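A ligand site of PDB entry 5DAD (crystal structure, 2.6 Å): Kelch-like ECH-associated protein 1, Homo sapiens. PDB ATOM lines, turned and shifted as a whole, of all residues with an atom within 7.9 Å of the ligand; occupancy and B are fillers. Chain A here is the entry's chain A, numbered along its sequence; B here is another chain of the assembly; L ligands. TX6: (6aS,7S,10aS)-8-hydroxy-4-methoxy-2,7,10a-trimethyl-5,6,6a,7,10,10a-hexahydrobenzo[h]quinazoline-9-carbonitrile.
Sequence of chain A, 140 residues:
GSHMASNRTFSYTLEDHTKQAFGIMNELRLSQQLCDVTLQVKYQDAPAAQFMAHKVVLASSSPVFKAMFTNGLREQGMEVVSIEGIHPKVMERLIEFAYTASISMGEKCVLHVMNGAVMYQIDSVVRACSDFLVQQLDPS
SG of Cys 109 is covalently linked to C1 of the ligand (1.7 Å).
The backbone NH of Gly 106 sits at hydrogen-bond distance from an oxygen (O17) of the ligand (2.8 Å).
A ring nitrogen (ND1) of His 87 lies within hydrogen-bond range of the backbone NH (N) of Lys 89 (3.2 Å).
N of Phe 10 of chain B is in hydrogen-bond range of O of Met 105 (2.7 Å).
Residues that only touch the ligand: His 87, Lys 108, Met 105, Tyr 43, His 112, Val 90 and Lys 89.
Hydrophobic or aromatic side chains that line the ligand: Tyr 43, His 87, Val 90, Met 105 and His 112.
Of the 24 residues printed, 9 come within 4 Å of the ligand.
Along chain A the residues within 4 Å of the ligand span positions 43 to 112.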
ATOM      1  N   TYR A  43      21.905  16.041  -2.890  1.00  0.00           N
ATOM      2  CA  TYR A  43      22.873  17.063  -2.506  1.00  0.00           C
ATOM      3  C   TYR A  43      22.474  17.672  -1.164  1.00  0.00           C
ATOM      4  O   TYR A  43      21.302  17.612  -0.777  1.00  0.00           O
ATOM      5  CB  TYR A  43      22.930  18.146  -3.602  1.00  0.00           C
ATOM      6  CG  TYR A  43      24.008  19.189  -3.426  1.00  0.00           C
ATOM      7  CD1 TYR A  43      25.352  18.885  -3.620  1.00  0.00           C
ATOM      8  CD2 TYR A  43      23.673  20.496  -3.082  1.00  0.00           C
ATOM      9  CE1 TYR A  43      26.345  19.842  -3.459  1.00  0.00           C
ATOM     10  CE2 TYR A  43      24.655  21.466  -2.923  1.00  0.00           C
ATOM     11  CZ  TYR A  43      25.979  21.132  -3.121  1.00  0.00           C
ATOM     12  OH  TYR A  43      26.948  22.108  -2.959  1.00  0.00           O
ATOM     13  N   GLN A  44      23.457  18.227  -0.456  1.00  0.00           N
ATOM     14  CA  GLN A  44      23.254  18.833   0.865  1.00  0.00           C
ATOM     15  C   GLN A  44      22.066  19.790   0.902  1.00  0.00           C
ATOM     16  O   GLN A  44      21.925  20.652   0.024  1.00  0.00           O
ATOM     17  CB  GLN A  44      24.535  19.536   1.342  1.00  0.00           C
ATOM     18  CG  GLN A  44      24.943  20.735   0.499  1.00  0.00           C
ATOM     19  CD  GLN A  44      26.415  21.084   0.619  1.00  0.00           C
ATOM     20  OE1 GLN A  44      27.282  20.215   0.580  1.00  0.00           O
ATOM     21  NE2 GLN A  44      26.701  22.376   0.749  1.00  0.00           N
ATOM     22  N   ALA A  46      19.328  20.604  -0.221  1.00  0.00           N
ATOM     23  CA  ALA A  46      18.440  20.614  -1.382  1.00  0.00           C
ATOM     24  C   ALA A  46      17.654  19.312  -1.587  1.00  0.00           C
ATOM     25  O   ALA A  46      18.194  18.226  -1.363  1.00  0.00           O
ATOM     26  CB  ALA A  46      19.232  20.956  -2.644  1.00  0.00           C
ATOM     27  N   ILE A  86      26.818  17.343  -6.544  1.00  0.00           N
ATOM     28  CA  ILE A  86      26.385  18.387  -7.473  1.00  0.00           C
ATOM     29  C   ILE A  86      24.921  18.764  -7.211  1.00  0.00           C
ATOM     30  O   ILE A  86      24.067  17.896  -7.031  1.00  0.00           O
ATOM     31  CB  ILE A  86      26.616  17.979  -8.958  1.00  0.00           C
ATOM     32  CG1 ILE A  86      26.386  19.178  -9.895  1.00  0.00           C
ATOM     33  CG2 ILE A  86      25.755  16.789  -9.351  1.00  0.00           C
ATOM     34  CD1 ILE A  86      26.690  18.895 -11.344  1.00  0.00           C
ATOM     35  N   HIS A  87      24.666  20.078  -7.163  1.00  0.00           N
ATOM     36  CA  HIS A  87      23.326  20.612  -6.953  1.00  0.00           C
ATOM     37  C   HIS A  87      22.408  20.282  -8.108  1.00  0.00           C
ATOM     38  O   HIS A  87      22.803  20.427  -9.268  1.00  0.00           O
ATOM     39  CB  HIS A  87      23.393  22.122  -6.739  1.00  0.00           C
ATOM     40  CG  HIS A  87      22.089  22.721  -6.271  1.00  0.00           C
ATOM     41  ND1 HIS A  87      21.188  23.252  -7.119  1.00  0.00           N
ATOM     42  CD2 HIS A  87      21.540  22.848  -4.999  1.00  0.00           C
ATOM     43  CE1 HIS A  87      20.127  23.701  -6.434  1.00  0.00           C
ATOM     44  NE2 HIS A  87      20.342  23.448  -5.134  1.00  0.00           N
ATOM     45  N   PRO A  88      21.167  19.833  -7.810  1.00  0.00           N
ATOM     46  CA  PRO A  88      20.242  19.400  -8.856  1.00  0.00           C
ATOM     47  C   PRO A  88      20.000  20.435  -9.954  1.00  0.00           C
ATOM     48  O   PRO A  88      19.917  20.074 -11.137  1.00  0.00           O
ATOM     49  CB  PRO A  88      18.944  19.140  -8.076  1.00  0.00           C
ATOM     50  CG  PRO A  88      19.406  18.777  -6.705  1.00  0.00           C
ATOM     51  CD  PRO A  88      20.597  19.652  -6.468  1.00  0.00           C
ATOM     52  N   LYS A  89      19.912  21.705  -9.578  1.00  0.00           N
ATOM     53  CA  LYS A  89      19.679  22.791 -10.531  1.00  0.00           C
ATOM     54  C   LYS A  89      20.898  23.010 -11.435  1.00  0.00           C
ATOM     55  O   LYS A  89      20.740  23.459 -12.572  1.00  0.00           O
ATOM     56  CB  LYS A  89      19.328  24.083  -9.779  1.00  0.00           C
ATOM     57  CG  LYS A  89      18.631  25.156 -10.610  1.00  0.00           C
ATOM     58  CD  LYS A  89      18.203  26.306  -9.708  1.00  0.00           C
ATOM     59  CE  LYS A  89      17.532  27.435 -10.483  1.00  0.00           C
ATOM     60  NZ  LYS A  89      17.167  28.572  -9.589  1.00  0.00           N
ATOM     61  N   VAL A  90      22.084  22.687 -10.936  1.00  0.00           N
ATOM     62  CA  VAL A  90      23.318  22.724 -11.730  1.00  0.00           C
ATOM     63  C   VAL A  90      23.300  21.614 -12.780  1.00  0.00           C
ATOM     64  O   VAL A  90      23.608  21.853 -13.948  1.00  0.00           O
ATOM     65  CB  VAL A  90      24.588  22.621 -10.852  1.00  0.00           C
ATOM     66  CG1 VAL A  90      25.851  22.563 -11.698  1.00  0.00           C
ATOM     67  CG2 VAL A  90      24.674  23.798  -9.878  1.00  0.00           C
ATOM     68  N   MET A  91      22.926  20.407 -12.357  1.00  0.00           N
ATOM     69  CA  MET A  91      22.797  19.260 -13.255  1.00  0.00           C
ATOM     70  C   MET A  91      21.771  19.546 -14.353  1.00  0.00           C
ATOM     71  O   MET A  91      22.019  19.285 -15.526  1.00  0.00           O
ATOM     72  CB  MET A  91      22.420  17.996 -12.470  1.00  0.00           C
ATOM     73  CG  MET A  91      22.421  16.718 -13.295  1.00  0.00           C
ATOM     74  SD  MET A  91      24.064  16.073 -13.713  1.00  0.00           S
ATOM     75  CE  MET A  91      24.419  16.926 -15.247  1.00  0.00           C
ATOM     76  N   GLU A  92      20.626  20.101 -13.939  1.00  0.00           N
ATOM     77  CA  GLU A  92      19.567  20.527 -14.857  1.00  0.00           C
ATOM     78  C   GLU A  92      20.104  21.441 -15.966  1.00  0.00           C
ATOM     79  O   GLU A  92      19.795  21.241 -17.135  1.00  0.00           O
ATOM     80  CB  GLU A  92      18.445  21.219 -14.082  1.00  0.00           C
ATOM     81  CG  GLU A  92      17.145  21.404 -14.846  1.00  0.00           C
ATOM     82  CD  GLU A  92      15.960  21.721 -13.949  1.00  0.00           C
ATOM     83  OE1 GLU A  92      16.022  22.718 -13.199  1.00  0.00           O
ATOM     84  OE2 GLU A  92      14.957  20.975 -14.008  1.00  0.00           O
ATOM     85  N   ARG A  93      20.911  22.431 -15.584  1.00  0.00           N
ATOM     86  CA  ARG A  93      21.475  23.381 -16.540  1.00  0.00           C
ATOM     87  C   ARG A  93      22.477  22.767 -17.507  1.00  0.00           C
ATOM     88  O   ARG A  93      22.592  23.206 -18.656  1.00  0.00           O
ATOM     89  CB  ARG A  93      22.103  24.579 -15.825  1.00  0.00           C
ATOM     90  CG  ARG A  93      21.124  25.485 -15.092  1.00  0.00           C
ATOM     91  CD  ARG A  93      20.131  26.167 -16.019  1.00  0.00           C
ATOM     92  NE  ARG A  93      19.151  26.953 -15.269  1.00  0.00           N
ATOM     93  CZ  ARG A  93      18.000  26.468 -14.786  1.00  0.00           C
ATOM     94  NH1 ARG A  93      17.667  25.194 -14.954  1.00  0.00           N
ATOM     95  NH2 ARG A  93      17.191  27.267 -14.110  1.00  0.00           N
ATOM     96  N   ILE A 103      23.243  27.618 -22.168  1.00  0.00           N
ATOM     97  CA  ILE A 103      23.148  27.559 -20.708  1.00  0.00           C
ATOM     98  C   ILE A 103      23.089  28.969 -20.158  1.00  0.00           C
ATOM     99  O   ILE A 103      23.777  29.878 -20.650  1.00  0.00           O
ATOM    100  CB  ILE A 103      24.312  26.747 -20.080  1.00  0.00           C
ATOM    101  CG1 ILE A 103      24.003  26.362 -18.634  1.00  0.00           C
ATOM    102  CG2 ILE A 103      25.645  27.487 -20.193  1.00  0.00           C
ATOM    103  CD1 ILE A 103      24.976  25.380 -18.020  1.00  0.00           C
ATOM    104  N   SER A 104      22.243  29.156 -19.152  1.00  0.00           N
ATOM    105  CA  SER A 104      22.125  30.436 -18.462  1.00  0.00           C
ATOM    106  C   SER A 104      22.030  30.209 -16.965  1.00  0.00           C
ATOM    107  O   SER A 104      21.524  29.176 -16.511  1.00  0.00           O
ATOM    108  CB  SER A 104      20.926  31.239 -18.970  1.00  0.00           C
ATOM    109  OG  SER A 104      19.705  30.639 -18.568  1.00  0.00           O
ATOM    110  N   MET A 105      22.513  31.184 -16.203  1.00  0.00           N
ATOM    111  CA  MET A 105      22.564  31.085 -14.754  1.00  0.00           C
ATOM    112  C   MET A 105      22.606  32.488 -14.180  1.00  0.00           C
ATOM    113  O   MET A 105      23.023  33.429 -14.863  1.00  0.00           O
ATOM    114  CB  MET A 105      23.824  30.300 -14.332  1.00  0.00           C
ATOM    115  CG  MET A 105      25.133  31.013 -14.643  1.00  0.00           C
ATOM    116  SD  MET A 105      26.448  29.983 -15.299  1.00  0.00           S
ATOM    117  CE  MET A 105      25.879  29.702 -16.978  1.00  0.00           C
ATOM    118  N   GLY A 106      22.174  32.625 -12.930  1.00  0.00           N
ATOM    119  CA  GLY A 106      22.273  33.895 -12.218  1.00  0.00           C
ATOM    120  C   GLY A 106      23.724  34.276 -11.983  1.00  0.00           C
ATOM    121  O   GLY A 106      24.545  33.433 -11.621  1.00  0.00           O
ATOM    122  N   GLU A 107      24.024  35.558 -12.176  1.00  0.00           N
ATOM    123  CA  GLU A 107      25.365  36.115 -12.007  1.00  0.00           C
ATOM    124  C   GLU A 107      26.091  35.571 -10.777  1.00  0.00           C
ATOM    125  O   GLU A 107      27.302  35.307 -10.818  1.00  0.00           O
ATOM    126  CB  GLU A 107      25.253  37.636 -11.903  1.00  0.00           C
ATOM    127  CG  GLU A 107      26.503  38.421 -12.270  1.00  0.00           C
ATOM    128  CD  GLU A 107      26.275  39.925 -12.247  1.00  0.00           C
ATOM    129  OE1 GLU A 107      25.441  40.393 -11.433  1.00  0.00           O
ATOM    130  OE2 GLU A 107      26.941  40.644 -13.023  1.00  0.00           O
ATOM    131  N   LYS A 108      25.345  35.380  -9.691  1.00  0.00           N
ATOM    132  CA  LYS A 108      25.924  34.996  -8.401  1.00  0.00           C
ATOM    133  C   LYS A 108      26.205  33.502  -8.239  1.00  0.00           C
ATOM    134  O   LYS A 108      26.711  33.077  -7.205  1.00  0.00           O
ATOM    135  CB  LYS A 108      25.032  35.496  -7.250  1.00  0.00           C
ATOM    136  CG  LYS A 108      23.588  35.000  -7.319  1.00  0.00           C
ATOM    137  CD  LYS A 108      23.010  34.778  -5.925  1.00  0.00           C
ATOM    138  CE  LYS A 108      21.623  34.170  -6.017  1.00  0.00           C
ATOM    139  NZ  LYS A 108      21.276  33.409  -4.772  1.00  0.00           N
ATOM    140  N   CYS A 109      25.860  32.713  -9.256  1.00  0.00           N
ATOM    141  CA  CYS A 109      26.019  31.250  -9.199  1.00  0.00           C
ATOM    142  C   CYS A 109      26.930  30.695 -10.287  1.00  0.00           C
ATOM    143  O   CYS A 109      27.089  29.480 -10.405  1.00  0.00           O
ATOM    144  CB  CYS A 109      24.652  30.566  -9.267  1.00  0.00           C
ATOM    145  SG  CYS A 109      23.803  30.557  -7.719  1.00  0.00           S
ATOM    146  N   VAL A 110      27.528  31.578 -11.082  1.00  0.00           N
ATOM    147  CA  VAL A 110      28.433  31.198 -12.175  1.00  0.00           C
ATOM    148  C   VAL A 110      29.507  30.210 -11.716  1.00  0.00           C
ATOM    149  O   VAL A 110      29.835  29.254 -12.421  1.00  0.00           O
ATOM    150  CB  VAL A 110      29.060  32.448 -12.835  1.00  0.00           C
ATOM    151  CG1 VAL A 110      30.179  32.058 -13.798  1.00  0.00           C
ATOM    152  CG2 VAL A 110      28.000  33.256 -13.564  1.00  0.00           C
ATOM    153  N   HIS A 112      29.250  28.014  -9.218  1.00  0.00           N
ATOM    154  CA  HIS A 112      28.636  26.723  -8.941  1.00  0.00           C
ATOM    155  C   HIS A 112      28.465  25.891 -10.180  1.00  0.00           C
ATOM    156  O   HIS A 112      28.711  24.680 -10.170  1.00  0.00           O
ATOM    157  CB  HIS A 112      27.297  26.905  -8.240  1.00  0.00           C
ATOM    158  CG  HIS A 112      27.415  27.332  -6.799  1.00  0.00           C
ATOM    159  ND1 HIS A 112      27.207  28.597  -6.393  1.00  0.00           N
ATOM    160  CD2 HIS A 112      27.738  26.601  -5.653  1.00  0.00           C
ATOM    161  CE1 HIS A 112      27.386  28.676  -5.064  1.00  0.00           C
ATOM    162  NE2 HIS A 112      27.710  27.452  -4.609  1.00  0.00           N
ATOM    163  N   VAL A 113      28.061  26.550 -11.267  1.00  0.00           N
ATOM    164  CA  VAL A 113      27.866  25.908 -12.559  1.00  0.00           C
ATOM    165  C   VAL A 113      29.215  25.444 -13.123  1.00  0.00           C
ATOM    166  O   VAL A 113      29.322  24.336 -13.671  1.00  0.00           O
ATOM    167  CB  VAL A 113      27.114  26.840 -13.537  1.00  0.00           C
ATOM    168  CG1 VAL A 113      27.011  26.222 -14.929  1.00  0.00           C
ATOM    169  CG2 VAL A 113      25.734  27.169 -13.003  1.00  0.00           C
ATOM    170  N   ARG B   8      21.138  40.323 -12.365  1.00  0.00           N
ATOM    171  CA  ARG B   8      21.736  39.979 -13.685  1.00  0.00           C
ATOM    172  C   ARG B   8      21.930  38.469 -13.832  1.00  0.00           C
ATOM    173  O   ARG B   8      22.110  37.761 -12.838  1.00  0.00           O
ATOM    174  CB  ARG B   8      23.060  40.714 -13.881  1.00  0.00           C
ATOM    175  N   THR B   9      21.884  37.980 -15.079  1.00  0.00           N
ATOM    176  CA  THR B   9      22.079  36.561 -15.385  1.00  0.00           C
ATOM    177  C   THR B   9      23.096  36.353 -16.508  1.00  0.00           C
ATOM    178  O   THR B   9      23.023  37.002 -17.548  1.00  0.00           O
ATOM    179  CB  THR B   9      20.757  35.849 -15.771  1.00  0.00           C
ATOM    180  OG1 THR B   9      20.231  36.430 -16.967  1.00  0.00           O
ATOM    181  CG2 THR B   9      19.719  35.932 -14.652  1.00  0.00           C
ATOM    182  N   PHE B  10      24.033  35.422 -16.289  1.00  0.00           N
ATOM    183  CA  PHE B  10      25.000  35.049 -17.310  1.00  0.00           C
ATOM    184  C   PHE B  10      24.404  33.987 -18.237  1.00  0.00           C
ATOM    185  O   PHE B  10      23.746  33.052 -17.777  1.00  0.00           O
ATOM    186  CB  PHE B  10      26.297  34.533 -16.665  1.00  0.00           C
ATOM    187  CG  PHE B  10      27.341  34.090 -17.661  1.00  0.00           C
ATOM    188  CD1 PHE B  10      27.922  34.990 -18.546  1.00  0.00           C
ATOM    189  CD2 PHE B  10      27.757  32.760 -17.687  1.00  0.00           C
ATOM    190  CE1 PHE B  10      28.886  34.579 -19.462  1.00  0.00           C
ATOM    191  CE2 PHE B  10      28.719  32.341 -18.599  1.00  0.00           C
ATOM    192  CZ  PHE B  10      29.280  33.255 -19.491  1.00  0.00           C
HETATM  193  N16 TX6 L   1      21.004  33.035  -9.282  1.00  0.00           N
HETATM  194  C15 TX6 L   1      21.275  31.903  -9.355  1.00  0.00           C
HETATM  195  C2  TX6 L   1      21.548  30.677  -9.292  1.00  0.00           C
HETATM  196  C1  TX6 L   1      22.127  30.162  -8.005  1.00  0.00           C
HETATM  197  C10 TX6 L   1      21.682  28.756  -7.644  1.00  0.00           C
HETATM  198  C19 TX6 L   1      20.174  28.716  -7.355  1.00  0.00           C
HETATM  199  C9  TX6 L   1      22.375  28.255  -6.395  1.00  0.00           C
HETATM  200  N11 TX6 L   1      22.362  29.034  -5.279  1.00  0.00           N
HETATM  201  C12 TX6 L   1      22.951  28.644  -4.127  1.00  0.00           C
HETATM  202  C20 TX6 L   1      22.931  29.534  -2.916  1.00  0.00           C
HETATM  203  N13 TX6 L   1      23.568  27.441  -4.060  1.00  0.00           N
HETATM  204  C14 TX6 L   1      23.611  26.619  -5.129  1.00  0.00           C
HETATM  205  O21 TX6 L   1      24.252  25.406  -5.043  1.00  0.00           O
HETATM  206  C22 TX6 L   1      24.981  25.028  -3.874  1.00  0.00           C
HETATM  207  C8  TX6 L   1      23.006  27.010  -6.332  1.00  0.00           C
HETATM  208  C7  TX6 L   1      23.058  26.076  -7.520  1.00  0.00           C
HETATM  209  C6  TX6 L   1      21.989  26.418  -8.560  1.00  0.00           C
HETATM  210  C5  TX6 L   1      22.071  27.904  -8.873  1.00  0.00           C
HETATM  211  C4  TX6 L   1      21.345  28.346 -10.166  1.00  0.00           C
HETATM  212  C18 TX6 L   1      21.973  27.697 -11.403  1.00  0.00           C
HETATM  213  C3  TX6 L   1      21.346  29.851 -10.337  1.00  0.00           C
HETATM  214  O17 TX6 L   1      21.128  30.375 -11.547  1.00  0.00           O
